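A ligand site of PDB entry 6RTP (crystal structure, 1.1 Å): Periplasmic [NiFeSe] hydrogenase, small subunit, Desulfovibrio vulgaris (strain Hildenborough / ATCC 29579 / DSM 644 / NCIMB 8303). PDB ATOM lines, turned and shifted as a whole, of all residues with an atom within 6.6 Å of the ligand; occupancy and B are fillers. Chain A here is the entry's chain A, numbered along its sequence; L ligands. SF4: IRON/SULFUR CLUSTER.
SG of Cys 211 lies close to N of Tyr 213, 3.4 Å away.
The backbone NH (N) of Tyr 234 lies close to the side-chain sulfur (SG) of Cys 232 (3.3 Å).
The guanidinium group (NE) of Arg 233 is in hydrogen-bond range of the backbone carbonyl oxygen (O) of Val 260, 2.9 Å away.
N of His 208 lies within hydrogen-bond range of O of Gly 240 (3.4 Å).
OH of Tyr 213 lies within hydrogen-bond range of NH2 of Arg 233.
The guanidinium group of Arg 233 sits at hydrogen-bond distance from the backbone carbonyl oxygen of Gly 231 (2.7 Å).
SD of Met 222 lies close to SG of Cys 232, 3.6 Å away.
N of Cys 238 lies within hydrogen-bond range of O of Arg 233, 3.2 Å away.
O of Tyr 213 sits close to S1 of the ligand (3.7 Å).
Tyr 217 touches the ligand (CB to S1, 3.8 Å).
Tyr 234 touches the ligand (CB to S4, 3.7 Å).
Gly 240 touches the ligand.
CD of Pro 241 touches S4 of the ligand (3.9 Å).
Val 260 touches the ligand (CG1 to S2, 3.6 Å).
Hydrophobic or aromatic side chains within 4 Å of the ligand: His 208, Tyr 217, Tyr 234, Pro 241 and Val 260.
12 residues have an atom within 4 Å of the ligand: His 208, Cys 211, Tyr 213, Leu 214, Tyr 217, Cys 232, Arg 233, Tyr 234, Cys 238, Gly 240, Pro 241 and Val 260.
The nearest printed residue that does not touch the ligand is Ile 207 (4.1 Å).
A ring nitrogen (ND1) of His 208 is bound to an iron atom (FE2) of the ligand (2.0 Å).
SG of Cys 232 binds FE3 of the ligand, 2.3 Å away.
The side-chain sulfur (SG) of Cys 211 binds an iron atom (FE4) of the ligand (2.3 Å).
The side-chain sulfur (SG) of Cys 238 binds an iron atom (FE1) of the ligand (2.3 Å).
S1 of the ligand lies close to N of Leu 214 (3.6 Å).
N of Arg 233 lies close to S2 of the ligand, 3.4 Å away.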
ATOM      1  N   ILE A 207      18.555   7.339  16.728  1.00  0.00           N
ATOM      2  CA  ILE A 207      17.936   6.823  15.506  1.00  0.00           C
ATOM      3  C   ILE A 207      18.853   5.823  14.808  1.00  0.00           C
ATOM      4  O   ILE A 207      18.480   4.679  14.509  1.00  0.00           O
ATOM      5  CB  ILE A 207      17.540   7.985  14.571  1.00  0.00           C
ATOM      6  CG1 ILE A 207      16.456   8.881  15.192  1.00  0.00           C
ATOM      7  CG2 ILE A 207      17.087   7.440  13.215  1.00  0.00           C
ATOM      8  CD1 ILE A 207      15.033   8.354  15.089  1.00  0.00           C
ATOM      9  N   HIS A 208      20.065   6.271  14.480  1.00  0.00           N
ATOM     10  CA  HIS A 208      20.980   5.492  13.638  1.00  0.00           C
ATOM     11  C   HIS A 208      21.318   4.148  14.255  1.00  0.00           C
ATOM     12  O   HIS A 208      21.348   3.130  13.553  1.00  0.00           O
ATOM     13  CB  HIS A 208      22.218   6.364  13.426  1.00  0.00           C
ATOM     14  CG  HIS A 208      23.346   5.691  12.735  1.00  0.00           C
ATOM     15  ND1 HIS A 208      23.422   5.553  11.365  1.00  0.00           N
ATOM     16  CD2 HIS A 208      24.501   5.175  13.231  1.00  0.00           C
ATOM     17  CE1 HIS A 208      24.559   4.965  11.046  1.00  0.00           C
ATOM     18  NE2 HIS A 208      25.234   4.718  12.168  1.00  0.00           N
ATOM     19  N   GLU A 209      21.612   4.120  15.560  1.00  0.00           N
ATOM     20  CA  GLU A 209      22.012   2.850  16.169  1.00  0.00           C
ATOM     21  C   GLU A 209      20.882   1.846  16.200  1.00  0.00           C
ATOM     22  O   GLU A 209      21.159   0.669  16.445  1.00  0.00           O
ATOM     23  CB  GLU A 209      22.592   3.065  17.571  1.00  0.00           C
ATOM     24  CG  GLU A 209      23.835   3.956  17.592  1.00  0.00           C
ATOM     25  CD  GLU A 209      24.998   3.419  16.753  1.00  0.00           C
ATOM     26  OE1 GLU A 209      25.112   2.192  16.555  1.00  0.00           O
ATOM     27  OE2 GLU A 209      25.825   4.237  16.285  1.00  0.00           O
ATOM     28  N   CYS A 211      18.589   1.814  13.493  1.00  0.00           N
ATOM     29  CA  CYS A 211      18.002   1.973  12.163  1.00  0.00           C
ATOM     30  C   CYS A 211      18.042   0.655  11.383  1.00  0.00           C
ATOM     31  O   CYS A 211      19.059  -0.053  11.404  1.00  0.00           O
ATOM     32  CB  CYS A 211      18.772   3.015  11.370  1.00  0.00           C
ATOM     33  SG  CYS A 211      18.099   3.284   9.720  1.00  0.00           S
ATOM     34  N   PRO A 212      16.974   0.327  10.647  1.00  0.00           N
ATOM     35  CA  PRO A 212      16.991  -0.901   9.859  1.00  0.00           C
ATOM     36  C   PRO A 212      18.004  -0.913   8.723  1.00  0.00           C
ATOM     37  O   PRO A 212      18.274  -1.986   8.178  1.00  0.00           O
ATOM     38  CB  PRO A 212      15.550  -1.013   9.328  1.00  0.00           C
ATOM     39  CG  PRO A 212      15.011   0.308   9.387  1.00  0.00           C
ATOM     40  CD  PRO A 212      15.670   1.000  10.570  1.00  0.00           C
ATOM     41  N   TYR A 213      18.571   0.239   8.346  1.00  0.00           N
ATOM     42  CA  TYR A 213      19.560   0.313   7.274  1.00  0.00           C
ATOM     43  C   TYR A 213      20.969   0.395   7.818  1.00  0.00           C
ATOM     44  O   TYR A 213      21.905   0.601   7.038  1.00  0.00           O
ATOM     45  CB  TYR A 213      19.235   1.483   6.322  1.00  0.00           C
ATOM     46  CG  TYR A 213      17.776   1.485   5.945  1.00  0.00           C
ATOM     47  CD1 TYR A 213      17.237   0.466   5.184  1.00  0.00           C
ATOM     48  CD2 TYR A 213      16.921   2.463   6.429  1.00  0.00           C
ATOM     49  CE1 TYR A 213      15.880   0.459   4.887  1.00  0.00           C
ATOM     50  CE2 TYR A 213      15.581   2.444   6.141  1.00  0.00           C
ATOM     51  CZ  TYR A 213      15.067   1.452   5.373  1.00  0.00           C
ATOM     52  OH  TYR A 213      13.709   1.486   5.123  1.00  0.00           O
ATOM     53  N   LEU A 214      21.149   0.164   9.121  1.00  0.00           N
ATOM     54  CA  LEU A 214      22.460   0.263   9.742  1.00  0.00           C
ATOM     55  C   LEU A 214      23.466  -0.707   9.113  1.00  0.00           C
ATOM     56  O   LEU A 214      24.637  -0.362   8.945  1.00  0.00           O
ATOM     57  CB  LEU A 214      22.340   0.018  11.236  1.00  0.00           C
ATOM     58  CG  LEU A 214      23.613   0.179  12.070  1.00  0.00           C
ATOM     59  CD1 LEU A 214      24.224   1.565  11.923  1.00  0.00           C
ATOM     60  CD2 LEU A 214      23.354  -0.136  13.529  1.00  0.00           C
ATOM     61  N   ASP A 215      23.031  -1.922   8.750  1.00  0.00           N
ATOM     62  CA  ASP A 215      23.937  -2.853   8.089  1.00  0.00           C
ATOM     63  C   ASP A 215      24.473  -2.259   6.796  1.00  0.00           C
ATOM     64  O   ASP A 215      25.654  -2.404   6.457  1.00  0.00           O
ATOM     65  CB  ASP A 215      23.225  -4.177   7.790  1.00  0.00           C
ATOM     66  CG  ASP A 215      22.984  -5.019   9.024  1.00  0.00           C
ATOM     67  OD1 ASP A 215      23.462  -4.655  10.124  1.00  0.00           O
ATOM     68  OD2 ASP A 215      22.289  -6.050   8.899  1.00  0.00           O
ATOM     69  N   LYS A 216      23.613  -1.587   6.028  1.00  0.00           N
ATOM     70  CA  LYS A 216      24.043  -0.986   4.769  1.00  0.00           C
ATOM     71  C   LYS A 216      25.022   0.146   5.023  1.00  0.00           C
ATOM     72  O   LYS A 216      26.014   0.289   4.308  1.00  0.00           O
ATOM     73  CB  LYS A 216      22.842  -0.488   3.973  1.00  0.00           C
ATOM     74  CG  LYS A 216      21.853  -1.588   3.638  1.00  0.00           C
ATOM     75  CD  LYS A 216      22.475  -2.683   2.816  1.00  0.00           C
ATOM     76  CE  LYS A 216      21.446  -3.736   2.496  1.00  0.00           C
ATOM     77  NZ  LYS A 216      22.033  -4.720   1.593  1.00  0.00           N
ATOM     78  N   TYR A 217      24.761   0.971   6.041  1.00  0.00           N
ATOM     79  CA  TYR A 217      25.720   2.010   6.421  1.00  0.00           C
ATOM     80  C   TYR A 217      27.087   1.400   6.690  1.00  0.00           C
ATOM     81  O   TYR A 217      28.107   1.856   6.155  1.00  0.00           O
ATOM     82  CB  TYR A 217      25.221   2.722   7.669  1.00  0.00           C
ATOM     83  CG  TYR A 217      26.189   3.739   8.222  1.00  0.00           C
ATOM     84  CD1 TYR A 217      26.164   5.069   7.808  1.00  0.00           C
ATOM     85  CD2 TYR A 217      27.114   3.372   9.201  1.00  0.00           C
ATOM     86  CE1 TYR A 217      27.049   5.981   8.333  1.00  0.00           C
ATOM     87  CE2 TYR A 217      27.993   4.281   9.718  1.00  0.00           C
ATOM     88  CZ  TYR A 217      27.958   5.590   9.284  1.00  0.00           C
ATOM     89  OH  TYR A 217      28.837   6.511   9.808  1.00  0.00           O
ATOM     90  N   ASP A 218      27.131   0.371   7.532  1.00  0.00           N
ATOM     91  CA  ASP A 218      28.407  -0.236   7.908  1.00  0.00           C
ATOM     92  C   ASP A 218      29.086  -0.876   6.704  1.00  0.00           C
ATOM     93  O   ASP A 218      30.316  -0.943   6.655  1.00  0.00           O
ATOM     94  CB  ASP A 218      28.215  -1.251   9.029  1.00  0.00           C
ATOM     95  CG  ASP A 218      27.897  -0.604  10.360  1.00  0.00           C
ATOM     96  OD1 ASP A 218      28.363   0.531  10.596  1.00  0.00           O
ATOM     97  OD2 ASP A 218      27.195  -1.241  11.181  1.00  0.00           O
ATOM     98  N   MET A 222      25.278   2.870  -0.121  1.00  0.00           N
ATOM     99  CA  MET A 222      24.568   4.138   0.013  1.00  0.00           C
ATOM    100  C   MET A 222      23.685   4.360  -1.201  1.00  0.00           C
ATOM    101  O   MET A 222      24.161   4.268  -2.331  1.00  0.00           O
ATOM    102  CB  MET A 222      25.571   5.285   0.062  1.00  0.00           C
ATOM    103  CG  MET A 222      26.510   5.214   1.242  1.00  0.00           C
ATOM    104  SD  MET A 222      25.569   5.448   2.759  1.00  0.00           S
ATOM    105  CE  MET A 222      26.887   5.192   3.960  1.00  0.00           C
ATOM    106  N   GLY A 231      19.599   0.932   0.018  1.00  0.00           N
ATOM    107  CA  GLY A 231      20.798   1.482   0.621  1.00  0.00           C
ATOM    108  C   GLY A 231      20.505   2.401   1.800  1.00  0.00           C
ATOM    109  O   GLY A 231      19.394   2.833   2.068  1.00  0.00           O
ATOM    110  N   CYS A 232      21.588   2.678   2.527  1.00  0.00           N
ATOM    111  CA  CYS A 232      21.554   3.698   3.577  1.00  0.00           C
ATOM    112  C   CYS A 232      21.410   5.081   2.944  1.00  0.00           C
ATOM    113  O   CYS A 232      21.865   5.321   1.811  1.00  0.00           O
ATOM    114  CB  CYS A 232      22.825   3.572   4.417  1.00  0.00           C
ATOM    115  SG  CYS A 232      23.239   4.967   5.504  1.00  0.00           S
ATOM    116  N   ARG A 233      20.774   5.992   3.692  1.00  0.00           N
ATOM    117  CA  ARG A 233      20.456   7.335   3.255  1.00  0.00           C
ATOM    118  C   ARG A 233      21.501   8.384   3.662  1.00  0.00           C
ATOM    119  O   ARG A 233      21.275   9.585   3.447  1.00  0.00           O
ATOM    120  CB  ARG A 233      19.082   7.730   3.824  1.00  0.00           C
ATOM    121  CG  ARG A 233      17.880   7.030   3.189  1.00  0.00           C
ATOM    122  CD  ARG A 233      17.756   5.544   3.488  1.00  0.00           C
ATOM    123  NE  ARG A 233      16.361   5.147   3.328  1.00  0.00           N
ATOM    124  CZ  ARG A 233      15.916   3.948   2.950  1.00  0.00           C
ATOM    125  NH1 ARG A 233      16.738   2.959   2.648  1.00  0.00           N
ATOM    126  NH2 ARG A 233      14.610   3.760   2.861  1.00  0.00           N
ATOM    127  N   TYR A 234      22.633   7.955   4.206  1.00  0.00           N
ATOM    128  CA  TYR A 234      23.629   8.890   4.717  1.00  0.00           C
ATOM    129  C   TYR A 234      24.118   9.873   3.642  1.00  0.00           C
ATOM    130  O   TYR A 234      24.202  11.078   3.899  1.00  0.00           O
ATOM    131  CB  TYR A 234      24.807   8.113   5.296  1.00  0.00           C
ATOM    132  CG  TYR A 234      25.880   8.975   5.889  1.00  0.00           C
ATOM    133  CD1 TYR A 234      25.737   9.511   7.156  1.00  0.00           C
ATOM    134  CD2 TYR A 234      27.039   9.263   5.198  1.00  0.00           C
ATOM    135  CE1 TYR A 234      26.701  10.287   7.703  1.00  0.00           C
ATOM    136  CE2 TYR A 234      28.020  10.049   5.739  1.00  0.00           C
ATOM    137  CZ  TYR A 234      27.848  10.566   6.998  1.00  0.00           C
ATOM    138  OH  TYR A 234      28.822  11.350   7.561  1.00  0.00           O
ATOM    139  N   ASP A 235      24.471   9.385   2.452  1.00  0.00           N
ATOM    140  CA  ASP A 235      24.976  10.302   1.433  1.00  0.00           C
ATOM    141  C   ASP A 235      23.904  11.264   0.942  1.00  0.00           C
ATOM    142  O   ASP A 235      24.252  12.345   0.439  1.00  0.00           O
ATOM    143  CB  ASP A 235      25.523   9.541   0.220  1.00  0.00           C
ATOM    144  CG  ASP A 235      26.858   8.874   0.476  1.00  0.00           C
ATOM    145  OD1 ASP A 235      27.466   9.103   1.546  1.00  0.00           O
ATOM    146  OD2 ASP A 235      27.309   8.114  -0.417  1.00  0.00           O
ATOM    147  N   CYS A 238      21.018  11.999   5.479  1.00  0.00           N
ATOM    148  CA  CYS A 238      20.382  11.537   6.713  1.00  0.00           C
ATOM    149  C   CYS A 238      21.182  11.955   7.940  1.00  0.00           C
ATOM    150  O   CYS A 238      22.387  11.685   8.032  1.00  0.00           O
ATOM    151  CB  CYS A 238      20.239  10.022   6.671  1.00  0.00           C
ATOM    152  SG  CYS A 238      19.297   9.373   8.078  1.00  0.00           S
ATOM    153  N   LYS A 239      20.492  12.560   8.911  1.00  0.00           N
ATOM    154  CA  LYS A 239      21.117  12.988  10.167  1.00  0.00           C
ATOM    155  C   LYS A 239      20.797  12.051  11.323  1.00  0.00           C
ATOM    156  O   LYS A 239      20.996  12.413  12.494  1.00  0.00           O
ATOM    157  CB  LYS A 239      20.697  14.408  10.520  1.00  0.00           C
ATOM    158  CG  LYS A 239      21.023  15.451   9.422  1.00  0.00           C
ATOM    159  CD  LYS A 239      22.458  15.377   8.920  1.00  0.00           C
ATOM    160  CE  LYS A 239      22.849  16.531   7.996  1.00  0.00           C
ATOM    161  NZ  LYS A 239      21.919  16.676   6.890  1.00  0.00           N
ATOM    162  N   GLY A 240      20.298  10.840  11.034  1.00  0.00           N
ATOM    163  CA  GLY A 240      20.062   9.871  12.078  1.00  0.00           C
ATOM    164  C   GLY A 240      21.216   9.672  13.034  1.00  0.00           C
ATOM    165  O   GLY A 240      20.989   9.492  14.238  1.00  0.00           O
ATOM    166  N   PRO A 241      22.460   9.697  12.575  1.00  0.00           N
ATOM    167  CA  PRO A 241      23.563   9.487  13.521  1.00  0.00           C
ATOM    168  C   PRO A 241      23.606  10.474  14.672  1.00  0.00           C
ATOM    169  O   PRO A 241      24.088  10.124  15.765  1.00  0.00           O
ATOM    170  CB  PRO A 241      24.805   9.577  12.624  1.00  0.00           C
ATOM    171  CG  PRO A 241      24.317   9.085  11.304  1.00  0.00           C
ATOM    172  CD  PRO A 241      22.938   9.668  11.171  1.00  0.00           C
ATOM    173  N   TRP A 258       7.912   6.710   7.987  1.00  0.00           N
ATOM    174  CA  TRP A 258       8.726   7.612   8.792  1.00  0.00           C
ATOM    175  C   TRP A 258       9.782   8.202   7.888  1.00  0.00           C
ATOM    176  O   TRP A 258       9.977   7.774   6.752  1.00  0.00           O
ATOM    177  CB  TRP A 258       9.346   6.949  10.023  1.00  0.00           C
ATOM    178  CG  TRP A 258      10.368   5.893   9.792  1.00  0.00           C
ATOM    179  CD1 TRP A 258      10.211   4.721   9.099  1.00  0.00           C
ATOM    180  CD2 TRP A 258      11.699   5.875  10.316  1.00  0.00           C
ATOM    181  NE1 TRP A 258      11.377   4.003   9.140  1.00  0.00           N
ATOM    182  CE2 TRP A 258      12.307   4.675   9.899  1.00  0.00           C
ATOM    183  CE3 TRP A 258      12.444   6.755  11.116  1.00  0.00           C
ATOM    184  CZ2 TRP A 258      13.614   4.323  10.252  1.00  0.00           C
ATOM    185  CZ3 TRP A 258      13.751   6.403  11.470  1.00  0.00           C
ATOM    186  CH2 TRP A 258      14.314   5.208  11.028  1.00  0.00           C
ATOM    187  N   VAL A 260      13.058   8.339   7.600  1.00  0.00           N
ATOM    188  CA  VAL A 260      14.197   7.628   7.034  1.00  0.00           C
ATOM    189  C   VAL A 260      13.740   6.670   5.941  1.00  0.00           C
ATOM    190  O   VAL A 260      14.414   6.525   4.916  1.00  0.00           O
ATOM    191  CB  VAL A 260      15.030   6.930   8.128  1.00  0.00           C
ATOM    192  CG1 VAL A 260      16.091   6.043   7.504  1.00  0.00           C
ATOM    193  CG2 VAL A 260      15.663   7.978   9.036  1.00  0.00           C
ATOM    194  N   ALA A 263      12.561   9.300   3.002  1.00  0.00           N
ATOM    195  CA  ALA A 263      13.536  10.243   2.487  1.00  0.00           C
ATOM    196  C   ALA A 263      14.761  10.226   3.394  1.00  0.00           C
ATOM    197  O   ALA A 263      15.535   9.259   3.336  1.00  0.00           O
ATOM    198  CB  ALA A 263      12.918  11.632   2.343  1.00  0.00           C
ATOM    199  N   CYS A 265      16.214  11.593   7.593  1.00  0.00           N
ATOM    200  CA  CYS A 265      16.011  12.315   8.849  1.00  0.00           C
ATOM    201  C   CYS A 265      16.748  13.646   8.765  1.00  0.00           C
ATOM    202  O   CYS A 265      17.884  13.695   8.289  1.00  0.00           O
ATOM    203  CB  CYS A 265      16.547  11.460  10.009  1.00  0.00           C
ATOM    204  SG  CYS A 265      16.536  12.268  11.652  1.00  0.00           S
HETATM  205 FE1  SF4 L   1      20.287   7.294   8.342  1.00  0.00          FE
HETATM  206 FE2  SF4 L   1      22.010   5.825   9.906  1.00  0.00          FE
HETATM  207 FE3  SF4 L   1      21.816   5.244   7.258  1.00  0.00          FE
HETATM  208 FE4  SF4 L   1      19.762   4.700   8.991  1.00  0.00          FE
HETATM  209  S1  SF4 L   1      21.821   3.721   8.963  1.00  0.00           S
HETATM  210  S2  SF4 L   1      19.594   5.607   6.890  1.00  0.00           S
HETATM  211  S3  SF4 L   1      19.901   6.488  10.450  1.00  0.00           S
HETATM  212  S4  SF4 L   1      22.571   7.242   8.175  1.00  0.00           S
